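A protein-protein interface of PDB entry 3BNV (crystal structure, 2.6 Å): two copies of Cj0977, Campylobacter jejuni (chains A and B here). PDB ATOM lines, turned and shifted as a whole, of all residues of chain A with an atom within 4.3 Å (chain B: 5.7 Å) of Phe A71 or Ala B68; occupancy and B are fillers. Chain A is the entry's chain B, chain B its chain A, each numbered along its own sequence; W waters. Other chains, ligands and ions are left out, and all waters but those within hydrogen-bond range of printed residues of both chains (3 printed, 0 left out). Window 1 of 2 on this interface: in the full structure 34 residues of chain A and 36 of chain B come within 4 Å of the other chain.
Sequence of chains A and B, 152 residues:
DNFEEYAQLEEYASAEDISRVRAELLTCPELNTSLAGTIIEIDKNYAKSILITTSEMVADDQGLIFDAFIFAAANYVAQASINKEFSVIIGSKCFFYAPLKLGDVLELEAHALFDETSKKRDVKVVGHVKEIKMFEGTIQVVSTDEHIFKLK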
ATOM      1  N   ASP A  67       9.700 -20.918  -2.806  1.00  0.00           N
ATOM      2  CA  ASP A  67      10.269 -20.613  -4.114  1.00  0.00           C
ATOM      3  C   ASP A  67      11.786 -20.519  -4.146  1.00  0.00           C
ATOM      4  O   ASP A  67      12.417 -20.820  -5.157  1.00  0.00           O
ATOM      5  CB  ASP A  67       9.617 -19.362  -4.696  1.00  0.00           C
ATOM      6  CG  ASP A  67       8.120 -19.576  -4.981  1.00  0.00           C
ATOM      7  OD1 ASP A  67       7.278 -18.725  -4.584  1.00  0.00           O
ATOM      8  OD2 ASP A  67       7.777 -20.625  -5.576  1.00  0.00           O
ATOM      9  N   ALA A  68      12.386 -20.143  -3.027  1.00  0.00           N
ATOM     10  CA  ALA A  68      13.813 -19.921  -2.998  1.00  0.00           C
ATOM     11  C   ALA A  68      14.575 -21.217  -3.256  1.00  0.00           C
ATOM     12  O   ALA A  68      15.724 -21.192  -3.694  1.00  0.00           O
ATOM     13  CB  ALA A  68      14.204 -19.342  -1.686  1.00  0.00           C
ATOM     14  N   PHE A  69      13.973 -22.362  -2.971  1.00  0.00           N
ATOM     15  CA  PHE A  69      14.693 -23.590  -3.220  1.00  0.00           C
ATOM     16  C   PHE A  69      14.794 -23.838  -4.713  1.00  0.00           C
ATOM     17  O   PHE A  69      15.716 -24.487  -5.167  1.00  0.00           O
ATOM     18  CB  PHE A  69      14.053 -24.757  -2.480  1.00  0.00           C
ATOM     19  CG  PHE A  69      14.178 -24.661  -0.972  1.00  0.00           C
ATOM     20  CD1 PHE A  69      15.359 -24.998  -0.341  1.00  0.00           C
ATOM     21  CD2 PHE A  69      13.103 -24.205  -0.191  1.00  0.00           C
ATOM     22  CE1 PHE A  69      15.472 -24.891   1.042  1.00  0.00           C
ATOM     23  CE2 PHE A  69      13.211 -24.095   1.185  1.00  0.00           C
ATOM     24  CZ  PHE A  69      14.392 -24.443   1.806  1.00  0.00           C
ATOM     25  N   ILE A  70      13.865 -23.297  -5.493  1.00  0.00           N
ATOM     26  CA  ILE A  70      13.990 -23.416  -6.933  1.00  0.00           C
ATOM     27  C   ILE A  70      15.148 -22.522  -7.331  1.00  0.00           C
ATOM     28  O   ILE A  70      15.988 -22.901  -8.146  1.00  0.00           O
ATOM     29  CB  ILE A  70      12.722 -22.951  -7.668  1.00  0.00           C
ATOM     30  CG1 ILE A  70      11.625 -24.015  -7.584  1.00  0.00           C
ATOM     31  CG2 ILE A  70      13.033 -22.669  -9.126  1.00  0.00           C
ATOM     32  CD1 ILE A  70      11.186 -24.341  -6.166  1.00  0.00           C
ATOM     33  N   PHE A  71      15.211 -21.347  -6.726  1.00  0.00           N
ATOM     34  CA  PHE A  71      16.304 -20.437  -6.994  1.00  0.00           C
ATOM     35  C   PHE A  71      17.625 -21.070  -6.603  1.00  0.00           C
ATOM     36  O   PHE A  71      18.606 -20.981  -7.352  1.00  0.00           O
ATOM     37  CB  PHE A  71      16.126 -19.115  -6.255  1.00  0.00           C
ATOM     38  CG  PHE A  71      17.176 -18.122  -6.582  1.00  0.00           C
ATOM     39  CD1 PHE A  71      18.287 -17.961  -5.760  1.00  0.00           C
ATOM     40  CD2 PHE A  71      17.089 -17.360  -7.742  1.00  0.00           C
ATOM     41  CE1 PHE A  71      19.279 -17.051  -6.073  1.00  0.00           C
ATOM     42  CE2 PHE A  71      18.089 -16.444  -8.053  1.00  0.00           C
ATOM     43  CZ  PHE A  71      19.183 -16.307  -7.209  1.00  0.00           C
ATOM     44  N   ALA A  72      17.668 -21.718  -5.449  1.00  0.00           N
ATOM     45  CA  ALA A  72      18.899 -22.389  -5.047  1.00  0.00           C
ATOM     46  C   ALA A  72      19.356 -23.367  -6.126  1.00  0.00           C
ATOM     47  O   ALA A  72      20.528 -23.416  -6.474  1.00  0.00           O
ATOM     48  CB  ALA A  72      18.740 -23.115  -3.715  1.00  0.00           C
ATOM     49  N   ALA A  73      18.432 -24.159  -6.655  1.00  0.00           N
ATOM     50  CA  ALA A  73      18.792 -25.121  -7.664  1.00  0.00           C
ATOM     51  C   ALA A  73      19.348 -24.363  -8.849  1.00  0.00           C
ATOM     52  O   ALA A  73      20.394 -24.735  -9.394  1.00  0.00           O
ATOM     53  CB  ALA A  73      17.597 -25.965  -8.062  1.00  0.00           C
ATOM     54  N   ALA A  74      18.670 -23.287  -9.245  1.00  0.00           N
ATOM     55  CA  ALA A  74      19.094 -22.518 -10.424  1.00  0.00           C
ATOM     56  C   ALA A  74      20.462 -21.884 -10.188  1.00  0.00           C
ATOM     57  O   ALA A  74      21.305 -21.840 -11.081  1.00  0.00           O
ATOM     58  CB  ALA A  74      18.077 -21.460 -10.746  1.00  0.00           C
ATOM     59  N   ASN A  75      20.666 -21.426  -8.953  1.00  0.00           N
ATOM     60  CA  ASN A  75      21.932 -20.858  -8.533  1.00  0.00           C
ATOM     61  C   ASN A  75      23.046 -21.882  -8.703  1.00  0.00           C
ATOM     62  O   ASN A  75      24.104 -21.566  -9.221  1.00  0.00           O
ATOM     63  CB  ASN A  75      21.812 -20.444  -7.064  1.00  0.00           C
ATOM     64  CG  ASN A  75      23.020 -19.708  -6.552  1.00  0.00           C
ATOM     65  OD1 ASN A  75      24.071 -19.659  -7.200  1.00  0.00           O
ATOM     66  ND2 ASN A  75      22.884 -19.134  -5.376  1.00  0.00           N
ATOM     67  N   ILE A  89      27.748 -15.589  -7.436  1.00  0.00           N
ATOM     68  CA  ILE A  89      26.807 -14.876  -8.272  1.00  0.00           C
ATOM     69  C   ILE A  89      26.594 -13.444  -7.786  1.00  0.00           C
ATOM     70  O   ILE A  89      26.640 -13.170  -6.579  1.00  0.00           O
ATOM     71  CB  ILE A  89      25.466 -15.613  -8.467  1.00  0.00           C
ATOM     72  CG1 ILE A  89      24.539 -15.382  -7.303  1.00  0.00           C
ATOM     73  CG2 ILE A  89      25.664 -17.108  -8.806  1.00  0.00           C
ATOM     74  CD1 ILE A  89      23.133 -15.676  -7.706  1.00  0.00           C
ATOM     75  N   SER A  92      20.685 -11.535 -10.402  1.00  0.00           N
ATOM     76  CA  SER A  92      19.789 -12.450 -11.119  1.00  0.00           C
ATOM     77  C   SER A  92      18.492 -11.792 -11.504  1.00  0.00           C
ATOM     78  O   SER A  92      18.077 -10.808 -10.877  1.00  0.00           O
ATOM     79  CB  SER A  92      19.479 -13.703 -10.289  1.00  0.00           C
ATOM     80  OG  SER A  92      18.639 -13.396  -9.187  1.00  0.00           O
ATOM     81  N   CYS A  94      14.770 -13.549 -12.336  1.00  0.00           N
ATOM     82  CA  CYS A  94      14.034 -14.809 -12.399  1.00  0.00           C
ATOM     83  C   CYS A  94      12.546 -14.641 -12.644  1.00  0.00           C
ATOM     84  O   CYS A  94      11.945 -13.656 -12.206  1.00  0.00           O
ATOM     85  CB  CYS A  94      14.158 -15.520 -11.066  1.00  0.00           C
ATOM     86  SG  CYS A  94      15.849 -15.902 -10.681  1.00  0.00           S
ATOM     87  N   PHE B  66      26.428 -19.879   0.362  1.00  0.00           N
ATOM     88  CA  PHE B  66      25.759 -19.979  -0.914  1.00  0.00           C
ATOM     89  C   PHE B  66      24.784 -18.839  -1.041  1.00  0.00           C
ATOM     90  O   PHE B  66      23.970 -18.622  -0.144  1.00  0.00           O
ATOM     91  CB  PHE B  66      24.996 -21.279  -0.982  1.00  0.00           C
ATOM     92  CG  PHE B  66      24.546 -21.653  -2.354  1.00  0.00           C
ATOM     93  CD1 PHE B  66      23.234 -22.060  -2.579  1.00  0.00           C
ATOM     94  CD2 PHE B  66      25.442 -21.664  -3.417  1.00  0.00           C
ATOM     95  CE1 PHE B  66      22.819 -22.458  -3.838  1.00  0.00           C
ATOM     96  CE2 PHE B  66      25.040 -22.059  -4.674  1.00  0.00           C
ATOM     97  CZ  PHE B  66      23.721 -22.450  -4.892  1.00  0.00           C
ATOM     98  N   ASP B  67      24.839 -18.118  -2.160  1.00  0.00           N
ATOM     99  CA  ASP B  67      24.046 -16.909  -2.324  1.00  0.00           C
ATOM    100  C   ASP B  67      22.534 -17.142  -2.210  1.00  0.00           C
ATOM    101  O   ASP B  67      21.795 -16.269  -1.734  1.00  0.00           O
ATOM    102  CB  ASP B  67      24.394 -16.241  -3.645  1.00  0.00           C
ATOM    103  CG  ASP B  67      25.838 -15.704  -3.683  1.00  0.00           C
ATOM    104  OD1 ASP B  67      26.670 -16.168  -4.513  1.00  0.00           O
ATOM    105  OD2 ASP B  67      26.145 -14.782  -2.892  1.00  0.00           O
ATOM    106  N   ALA B  68      22.060 -18.315  -2.607  1.00  0.00           N
ATOM    107  CA  ALA B  68      20.630 -18.603  -2.568  1.00  0.00           C
ATOM    108  C   ALA B  68      20.014 -18.448  -1.190  1.00  0.00           C
ATOM    109  O   ALA B  68      18.820 -18.156  -1.064  1.00  0.00           O
ATOM    110  CB  ALA B  68      20.358 -19.978  -3.099  1.00  0.00           C
ATOM    111  N   PHE B  69      20.802 -18.621  -0.145  1.00  0.00           N
ATOM    112  CA  PHE B  69      20.245 -18.448   1.200  1.00  0.00           C
ATOM    113  C   PHE B  69      19.937 -17.002   1.472  1.00  0.00           C
ATOM    114  O   PHE B  69      18.995 -16.682   2.193  1.00  0.00           O
ATOM    115  CB  PHE B  69      21.144 -19.048   2.268  1.00  0.00           C
ATOM    116  CG  PHE B  69      21.245 -20.517   2.144  1.00  0.00           C
ATOM    117  CD1 PHE B  69      20.197 -21.310   2.539  1.00  0.00           C
ATOM    118  CD2 PHE B  69      22.329 -21.097   1.518  1.00  0.00           C
ATOM    119  CE1 PHE B  69      20.243 -22.672   2.390  1.00  0.00           C
ATOM    120  CE2 PHE B  69      22.393 -22.446   1.359  1.00  0.00           C
ATOM    121  CZ  PHE B  69      21.346 -23.247   1.792  1.00  0.00           C
ATOM    122  N   ILE B  70      20.707 -16.110   0.859  1.00  0.00           N
ATOM    123  CA  ILE B  70      20.396 -14.710   1.020  1.00  0.00           C
ATOM    124  C   ILE B  70      19.079 -14.493   0.311  1.00  0.00           C
ATOM    125  O   ILE B  70      18.196 -13.811   0.838  1.00  0.00           O
ATOM    126  CB  ILE B  70      21.437 -13.846   0.373  1.00  0.00           C
ATOM    127  CG1 ILE B  70      22.809 -14.152   0.934  1.00  0.00           C
ATOM    128  CG2 ILE B  70      21.134 -12.400   0.576  1.00  0.00           C
ATOM    129  CD1 ILE B  70      23.918 -13.548   0.001  1.00  0.00           C
ATOM    130  N   PHE B  71      18.935 -15.094  -0.876  1.00  0.00           N
ATOM    131  CA  PHE B  71      17.690 -14.955  -1.611  1.00  0.00           C
ATOM    132  C   PHE B  71      16.556 -15.541  -0.789  1.00  0.00           C
ATOM    133  O   PHE B  71      15.522 -14.918  -0.622  1.00  0.00           O
ATOM    134  CB  PHE B  71      17.746 -15.620  -2.980  1.00  0.00           C
ATOM    135  CG  PHE B  71      16.443 -15.507  -3.777  1.00  0.00           C
ATOM    136  CD1 PHE B  71      15.476 -16.487  -3.712  1.00  0.00           C
ATOM    137  CD2 PHE B  71      16.194 -14.407  -4.590  1.00  0.00           C
ATOM    138  CE1 PHE B  71      14.295 -16.375  -4.453  1.00  0.00           C
ATOM    139  CE2 PHE B  71      15.006 -14.296  -5.300  1.00  0.00           C
ATOM    140  CZ  PHE B  71      14.068 -15.285  -5.241  1.00  0.00           C
ATOM    141  N   ALA B  72      16.750 -16.731  -0.236  1.00  0.00           N
ATOM    142  CA  ALA B  72      15.708 -17.300   0.578  1.00  0.00           C
ATOM    143  C   ALA B  72      15.254 -16.315   1.636  1.00  0.00           C
ATOM    144  O   ALA B  72      14.062 -16.125   1.820  1.00  0.00           O
ATOM    145  CB  ALA B  72      16.169 -18.581   1.215  1.00  0.00           C
ATOM    146  N   ALA B  73      16.185 -15.691   2.340  1.00  0.00           N
ATOM    147  CA  ALA B  73      15.797 -14.773   3.387  1.00  0.00           C
ATOM    148  C   ALA B  73      14.985 -13.612   2.773  1.00  0.00           C
ATOM    149  O   ALA B  73      13.938 -13.226   3.293  1.00  0.00           O
ATOM    150  CB  ALA B  73      17.014 -14.285   4.115  1.00  0.00           C
ATOM    151  N   SER B  92      11.626 -12.125  -9.671  1.00  0.00           N
ATOM    152  CA  SER B  92      12.569 -11.318  -8.876  1.00  0.00           C
ATOM    153  C   SER B  92      13.711 -10.739  -9.692  1.00  0.00           C
ATOM    154  O   SER B  92      14.086 -11.266 -10.754  1.00  0.00           O
ATOM    155  CB  SER B  92      13.121 -12.106  -7.677  1.00  0.00           C
ATOM    156  OG  SER B  92      13.531 -13.389  -8.096  1.00  0.00           O
ATOM    157  N   PHE B  96      23.520  -8.988  -5.716  1.00  0.00           N
ATOM    158  CA  PHE B  96      24.321  -9.488  -4.614  1.00  0.00           C
ATOM    159  C   PHE B  96      25.650  -8.776  -4.625  1.00  0.00           C
ATOM    160  O   PHE B  96      26.545  -9.181  -5.339  1.00  0.00           O
ATOM    161  CB  PHE B  96      24.611 -10.961  -4.835  1.00  0.00           C
ATOM    162  CG  PHE B  96      23.382 -11.809  -4.939  1.00  0.00           C
ATOM    163  CD1 PHE B  96      22.780 -12.038  -6.163  1.00  0.00           C
ATOM    164  CD2 PHE B  96      22.847 -12.388  -3.829  1.00  0.00           C
ATOM    165  CE1 PHE B  96      21.669 -12.834  -6.247  1.00  0.00           C
ATOM    166  CE2 PHE B  96      21.742 -13.173  -3.914  1.00  0.00           C
ATOM    167  CZ  PHE B  96      21.155 -13.403  -5.120  1.00  0.00           C
HETATM  168  O   HOH W   1      27.588 -13.322  -4.252  1.00  0.00           O
HETATM  169  O   HOH W   2      26.379 -18.604  -4.962  1.00  0.00           O
HETATM  170  O   HOH W   3      16.087 -12.592  -8.821  1.00  0.00           O
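Of chain B, only Ala B68 and Phe B71 come within 4 Å of Phe A71.
Of the printed residues of chain B, Ala A72 touches Phe B66 and Ala B68.
Ala A73 touches none of the printed residues of chain B.
Ser A92 touches none of the printed residues of chain B.
Of the printed residues of chain A, Phe B66 touches Ala A72 and Asn A75.
Ala B68 touches three residues of chain A.
Of the printed residues of chain A, Ser B92 touches Cys A94.
The nearest printed residue of chain A that does not touch Ala B68 is Ala A68 (4.8 Å).
Of the 12 printed residues of chain A, 6 touch a printed residue of chain B.
Hydrophobic or aromatic side chains of chain A within 4 Å of the printed part of chain B: Ala A68, Phe A71, Ala A72 and Ile A89.
Of the 10 printed residues of chain B, 7 touch a printed residue of chain A.
Hydrophobic or aromatic side chains of chain B within 4 Å of the printed part of chain A: Phe B66, Ala B68, Phe B71, Ala B72 and Phe B96.
Among the printed residues, 12 pairs touch across the chains.
The backbone NH (N) of Ile A89 sits at hydrogen-bond distance from the side-chain carboxylate (OD1) of Asp B67, 3.2 Å away.
The backbone NH of Ala B68 lies close to the side-chain amide nitrogen of Asn A75, at 3.0 Å.
N of Cys A94 is in hydrogen-bond range of O of Ser B92, at 2.9 Å.
Ala A68 touches Phe B71, and with the chains exchanged Phe A71 touches Ala B68.
Ala A68 touches Ala B72, and with the chains exchanged Ala A72 touches Ala B68.
Phe A71 touches its own counterpart, Phe B71.
8 positions are printed for both chains.
Among the printed residues, merely in contact across the chains: Asn A75 with Phe B66 (3.3 Å), Ala A68 with Ala B72 (3.4 Å), Ala A72 with Ala B68 (3.4 Å), Ile A89 with Phe B96 (3.5 Å), Ala A72 with Phe B66 (3.6 Å), Phe A71 with Phe B71 (3.7 Å), Asn A75 with Asp B67 (3.7 Å), Ala A68 with Phe B71 (3.7 Å) and Phe A71 with Ala B68 (3.9 Å).
Water W1 bridges OD2 of Asp B67 and O of Ile A89.
Water W2 lies within hydrogen-bond range of OD1 of Asp B67 and OD1 of Asn A75.
Water W3 lies within hydrogen-bond range of the side-chain hydroxyl of Ser A92 (2.7 Å) and the side-chain hydroxyl of Ser B92 (2.8 Å).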
